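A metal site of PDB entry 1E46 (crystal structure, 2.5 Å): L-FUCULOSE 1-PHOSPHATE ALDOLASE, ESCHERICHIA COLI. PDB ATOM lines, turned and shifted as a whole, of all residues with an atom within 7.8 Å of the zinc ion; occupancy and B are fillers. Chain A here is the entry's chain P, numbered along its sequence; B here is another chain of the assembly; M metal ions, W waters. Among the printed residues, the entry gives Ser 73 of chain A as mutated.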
ATOM      1  N   ALA A  27      -6.839  -3.273  -3.644  1.00  0.00           N
ATOM      2  CA  ALA A  27      -6.672  -2.463  -4.824  1.00  0.00           C
ATOM      3  C   ALA A  27      -5.178  -2.163  -5.080  1.00  0.00           C
ATOM      4  O   ALA A  27      -4.699  -2.367  -6.201  1.00  0.00           O
ATOM      5  CB  ALA A  27      -7.395  -1.111  -4.710  1.00  0.00           C
ATOM      6  N   GLY A  28      -4.444  -1.676  -4.057  1.00  0.00           N
ATOM      7  CA  GLY A  28      -3.058  -1.326  -4.292  1.00  0.00           C
ATOM      8  C   GLY A  28      -2.012  -2.401  -4.139  1.00  0.00           C
ATOM      9  O   GLY A  28      -2.222  -3.461  -3.578  1.00  0.00           O
ATOM     10  N   ASN A  29      -0.788  -2.070  -4.552  1.00  0.00           N
ATOM     11  CA  ASN A  29       0.401  -2.874  -4.506  1.00  0.00           C
ATOM     12  C   ASN A  29       1.551  -2.009  -3.996  1.00  0.00           C
ATOM     13  O   ASN A  29       1.390  -0.812  -3.915  1.00  0.00           O
ATOM     14  CB  ASN A  29       0.785  -3.392  -5.876  1.00  0.00           C
ATOM     15  CG  ASN A  29       0.228  -2.568  -7.018  1.00  0.00           C
ATOM     16  OD1 ASN A  29       0.861  -1.708  -7.611  1.00  0.00           O
ATOM     17  ND2 ASN A  29      -1.044  -2.838  -7.359  1.00  0.00           N
ATOM     18  N   SER A  72      -0.479  -7.142 -11.123  1.00  0.00           N
ATOM     19  CA  SER A  72      -0.683  -6.775 -12.531  1.00  0.00           C
ATOM     20  C   SER A  72      -0.150  -5.360 -12.743  1.00  0.00           C
ATOM     21  O   SER A  72       0.223  -5.007 -13.853  1.00  0.00           O
ATOM     22  CB  SER A  72      -2.138  -6.989 -12.927  1.00  0.00           C
ATOM     23  OG  SER A  72      -3.016  -6.091 -12.235  1.00  0.00           O
ATOM     24  N   SER A  73       0.050  -4.587 -11.673  1.00  0.00           N
ATOM     25  CA  SER A  73       0.597  -3.244 -11.828  1.00  0.00           C
ATOM     26  C   SER A  73       2.114  -3.176 -11.906  1.00  0.00           C
ATOM     27  O   SER A  73       2.641  -2.079 -11.919  1.00  0.00           O
ATOM     28  CB  SER A  73       0.053  -2.410 -10.658  1.00  0.00           C
ATOM     29  OG  SER A  73      -1.316  -2.057 -10.876  1.00  0.00           O
ATOM     30  N   PHE A  76       4.364  -0.475 -14.356  1.00  0.00           N
ATOM     31  CA  PHE A  76       4.541   0.971 -14.127  1.00  0.00           C
ATOM     32  C   PHE A  76       5.231   1.249 -12.813  1.00  0.00           C
ATOM     33  O   PHE A  76       5.490   2.401 -12.396  1.00  0.00           O
ATOM     34  CB  PHE A  76       3.201   1.564 -14.404  1.00  0.00           C
ATOM     35  CG  PHE A  76       2.113   1.314 -13.417  1.00  0.00           C
ATOM     36  CD1 PHE A  76       2.268   1.538 -12.058  1.00  0.00           C
ATOM     37  CD2 PHE A  76       0.872   0.890 -13.895  1.00  0.00           C
ATOM     38  CE1 PHE A  76       1.195   1.363 -11.189  1.00  0.00           C
ATOM     39  CE2 PHE A  76      -0.203   0.662 -13.064  1.00  0.00           C
ATOM     40  CZ  PHE A  76      -0.006   0.941 -11.717  1.00  0.00           C
ATOM     41  N   HIS A  92       1.319   1.846  -4.810  1.00  0.00           N
ATOM     42  CA  HIS A  92       0.241   2.270  -5.749  1.00  0.00           C
ATOM     43  C   HIS A  92      -1.109   2.222  -5.040  1.00  0.00           C
ATOM     44  O   HIS A  92      -1.222   1.274  -4.273  1.00  0.00           O
ATOM     45  CB  HIS A  92       0.165   1.390  -6.988  1.00  0.00           C
ATOM     46  CG  HIS A  92      -1.076   1.467  -7.779  1.00  0.00           C
ATOM     47  ND1 HIS A  92      -1.490   2.639  -8.364  1.00  0.00           N
ATOM     48  CD2 HIS A  92      -2.031   0.578  -8.177  1.00  0.00           C
ATOM     49  CE1 HIS A  92      -2.603   2.498  -9.085  1.00  0.00           C
ATOM     50  NE2 HIS A  92      -2.937   1.240  -9.008  1.00  0.00           N
ATOM     51  N   ASN A  93      -2.149   2.993  -5.364  1.00  0.00           N
ATOM     52  CA  ASN A  93      -3.426   2.706  -4.731  1.00  0.00           C
ATOM     53  C   ASN A  93      -4.596   3.407  -5.368  1.00  0.00           C
ATOM     54  O   ASN A  93      -4.437   4.204  -6.275  1.00  0.00           O
ATOM     55  CB  ASN A  93      -3.290   2.976  -3.250  1.00  0.00           C
ATOM     56  CG  ASN A  93      -3.394   4.397  -2.760  1.00  0.00           C
ATOM     57  OD1 ASN A  93      -4.043   5.327  -3.296  1.00  0.00           O
ATOM     58  ND2 ASN A  93      -2.683   4.532  -1.611  1.00  0.00           N
ATOM     59  N   HIS A  94      -5.853   3.185  -4.961  1.00  0.00           N
ATOM     60  CA  HIS A  94      -7.030   3.833  -5.510  1.00  0.00           C
ATOM     61  C   HIS A  94      -7.715   4.560  -4.357  1.00  0.00           C
ATOM     62  O   HIS A  94      -8.902   4.285  -4.093  1.00  0.00           O
ATOM     63  CB  HIS A  94      -7.986   2.832  -6.152  1.00  0.00           C
ATOM     64  CG  HIS A  94      -7.428   1.945  -7.214  1.00  0.00           C
ATOM     65  ND1 HIS A  94      -7.858   0.687  -7.476  1.00  0.00           N
ATOM     66  CD2 HIS A  94      -6.412   2.113  -8.106  1.00  0.00           C
ATOM     67  CE1 HIS A  94      -7.136   0.135  -8.463  1.00  0.00           C
ATOM     68  NE2 HIS A  94      -6.229   0.998  -8.881  1.00  0.00           N
ATOM     69  N   PHE A 131      -4.999  -0.536 -18.445  1.00  0.00           N
ATOM     70  CA  PHE A 131      -4.053  -1.092 -17.462  1.00  0.00           C
ATOM     71  C   PHE A 131      -3.136  -2.127 -18.102  1.00  0.00           C
ATOM     72  O   PHE A 131      -3.400  -2.753 -19.136  1.00  0.00           O
ATOM     73  CB  PHE A 131      -4.664  -1.586 -16.176  1.00  0.00           C
ATOM     74  CG  PHE A 131      -5.744  -2.599 -16.179  1.00  0.00           C
ATOM     75  CD1 PHE A 131      -7.023  -2.291 -16.624  1.00  0.00           C
ATOM     76  CD2 PHE A 131      -5.493  -3.896 -15.711  1.00  0.00           C
ATOM     77  CE1 PHE A 131      -8.003  -3.272 -16.618  1.00  0.00           C
ATOM     78  CE2 PHE A 131      -6.462  -4.887 -15.676  1.00  0.00           C
ATOM     79  CZ  PHE A 131      -7.709  -4.525 -16.113  1.00  0.00           C
ATOM     80  N   LEU A 152      -3.480   9.073 -11.719  1.00  0.00           N
ATOM     81  CA  LEU A 152      -3.609   8.292 -12.964  1.00  0.00           C
ATOM     82  C   LEU A 152      -5.086   8.469 -13.386  1.00  0.00           C
ATOM     83  O   LEU A 152      -5.876   8.240 -12.454  1.00  0.00           O
ATOM     84  CB  LEU A 152      -3.231   6.854 -12.750  1.00  0.00           C
ATOM     85  CG  LEU A 152      -1.740   6.519 -12.974  1.00  0.00           C
ATOM     86  CD1 LEU A 152      -1.008   7.076 -11.765  1.00  0.00           C
ATOM     87  CD2 LEU A 152      -1.636   5.004 -12.874  1.00  0.00           C
ATOM     88  N   HIS A 155      -8.384   6.190 -12.568  1.00  0.00           N
ATOM     89  CA  HIS A 155      -7.688   5.011 -12.042  1.00  0.00           C
ATOM     90  C   HIS A 155      -7.289   5.180 -10.599  1.00  0.00           C
ATOM     91  O   HIS A 155      -7.777   4.390  -9.809  1.00  0.00           O
ATOM     92  CB  HIS A 155      -6.442   4.687 -12.868  1.00  0.00           C
ATOM     93  CG  HIS A 155      -5.778   3.388 -12.481  1.00  0.00           C
ATOM     94  ND1 HIS A 155      -5.069   2.644 -13.415  1.00  0.00           N
ATOM     95  CD2 HIS A 155      -5.679   2.716 -11.292  1.00  0.00           C
ATOM     96  CE1 HIS A 155      -4.594   1.574 -12.740  1.00  0.00           C
ATOM     97  NE2 HIS A 155      -4.950   1.559 -11.453  1.00  0.00           N
ATOM     98  N   GLY A 156      -6.274   5.984 -10.295  1.00  0.00           N
ATOM     99  CA  GLY A 156      -5.730   6.032  -8.923  1.00  0.00           C
ATOM    100  C   GLY A 156      -4.500   6.882  -8.678  1.00  0.00           C
ATOM    101  O   GLY A 156      -4.259   7.875  -9.312  1.00  0.00           O
ATOM    102  N   LEU A 157      -3.607   6.573  -7.762  1.00  0.00           N
ATOM    103  CA  LEU A 157      -2.432   7.260  -7.328  1.00  0.00           C
ATOM    104  C   LEU A 157      -1.188   6.412  -7.298  1.00  0.00           C
ATOM    105  O   LEU A 157      -1.286   5.236  -6.955  1.00  0.00           O
ATOM    106  CB  LEU A 157      -2.709   7.797  -5.906  1.00  0.00           C
ATOM    107  CG  LEU A 157      -1.660   8.228  -4.935  1.00  0.00           C
ATOM    108  CD1 LEU A 157      -0.910   7.175  -4.148  1.00  0.00           C
ATOM    109  CD2 LEU A 157      -0.871   9.460  -5.128  1.00  0.00           C
ATOM    110  N   ILE A 158      -0.018   6.964  -7.665  1.00  0.00           N
ATOM    111  CA  ILE A 158       1.262   6.256  -7.601  1.00  0.00           C
ATOM    112  C   ILE A 158       2.206   7.250  -6.895  1.00  0.00           C
ATOM    113  O   ILE A 158       2.292   8.362  -7.409  1.00  0.00           O
ATOM    114  CB  ILE A 158       2.038   5.879  -8.857  1.00  0.00           C
ATOM    115  CG1 ILE A 158       1.213   5.088  -9.868  1.00  0.00           C
ATOM    116  CG2 ILE A 158       3.318   5.086  -8.569  1.00  0.00           C
ATOM    117  CD1 ILE A 158       1.943   5.050 -11.208  1.00  0.00           C
ATOM    118  N   HIS B 112     -14.944   4.976 -13.812  1.00  0.00           N
ATOM    119  CA  HIS B 112     -13.703   4.246 -13.545  1.00  0.00           C
ATOM    120  C   HIS B 112     -13.775   2.814 -14.056  1.00  0.00           C
ATOM    121  O   HIS B 112     -14.814   2.026 -13.999  1.00  0.00           O
ATOM    122  CB  HIS B 112     -13.588   4.264 -12.022  1.00  0.00           C
ATOM    123  CG  HIS B 112     -12.340   3.768 -11.383  1.00  0.00           C
ATOM    124  ND1 HIS B 112     -12.021   2.429 -11.281  1.00  0.00           N
ATOM    125  CD2 HIS B 112     -11.308   4.484 -10.821  1.00  0.00           C
ATOM    126  CE1 HIS B 112     -10.856   2.342 -10.646  1.00  0.00           C
ATOM    127  NE2 HIS B 112     -10.385   3.571 -10.377  1.00  0.00           N
ATOM    128  N   TYR B 113     -12.598   2.343 -14.495  1.00  0.00           N
ATOM    129  CA  TYR B 113     -12.490   0.991 -15.040  1.00  0.00           C
ATOM    130  C   TYR B 113     -13.005  -0.061 -14.122  1.00  0.00           C
ATOM    131  O   TYR B 113     -13.422  -1.089 -14.743  1.00  0.00           O
ATOM    132  CB  TYR B 113     -11.136   0.634 -15.603  1.00  0.00           C
ATOM    133  CG  TYR B 113     -10.124   0.097 -14.637  1.00  0.00           C
ATOM    134  CD1 TYR B 113      -9.259   0.925 -13.922  1.00  0.00           C
ATOM    135  CD2 TYR B 113      -9.995  -1.285 -14.440  1.00  0.00           C
ATOM    136  CE1 TYR B 113      -8.337   0.451 -13.025  1.00  0.00           C
ATOM    137  CE2 TYR B 113      -9.069  -1.795 -13.538  1.00  0.00           C
ATOM    138  CZ  TYR B 113      -8.245  -0.908 -12.830  1.00  0.00           C
ATOM    139  OH  TYR B 113      -7.305  -1.464 -11.953  1.00  0.00           O
ATOM    140  N   MET B 114     -13.145   0.070 -12.804  1.00  0.00           N
ATOM    141  CA  MET B 114     -13.703  -1.023 -11.983  1.00  0.00           C
ATOM    142  C   MET B 114     -15.202  -1.201 -12.190  1.00  0.00           C
ATOM    143  O   MET B 114     -15.775  -2.230 -11.873  1.00  0.00           O
ATOM    144  CB  MET B 114     -13.385  -0.942 -10.509  1.00  0.00           C
ATOM    145  CG  MET B 114     -11.932  -1.205 -10.132  1.00  0.00           C
ATOM    146  SD  MET B 114     -11.373  -2.867 -10.607  1.00  0.00           S
ATOM    147  CE  MET B 114     -12.217  -3.882  -9.398  1.00  0.00           C
HETATM  148 ZN    ZN M   1      -4.577   0.107  -9.775  1.00  0.00          ZN
HETATM  149  O   HOH W   1      -4.690  -1.769  -9.746  1.00  0.00           O
HETATM  150  O   HOH W   2      -3.724  -1.984 -11.974  1.00  0.00           O
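The backbone NH (N) of His 92 lies within hydrogen-bond range of the backbone carbonyl oxygen (O) of Asn 29 (2.8 Å). A ring nitrogen (ND1) of His 92 sits at hydrogen-bond distance from the backbone carbonyl oxygen of Leu 157 (3.0 Å). A ring nitrogen (NE2) of His 112 of chain B lies within hydrogen-bond range of the backbone carbonyl oxygen of His 155, 2.8 Å away.
Tyr 113 of chain B touches the zinc ion (OH to ZN, 3.8 Å).
The zinc ion is bound by water W1 (1.9 Å), a ring nitrogen (NE2) of His 94 (2.1 Å), a ring nitrogen (NE2) of His 92 (2.1 Å) and a ring nitrogen (NE2) of His 155 (2.3 Å). The zinc ion has four donor atoms within binding distance.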
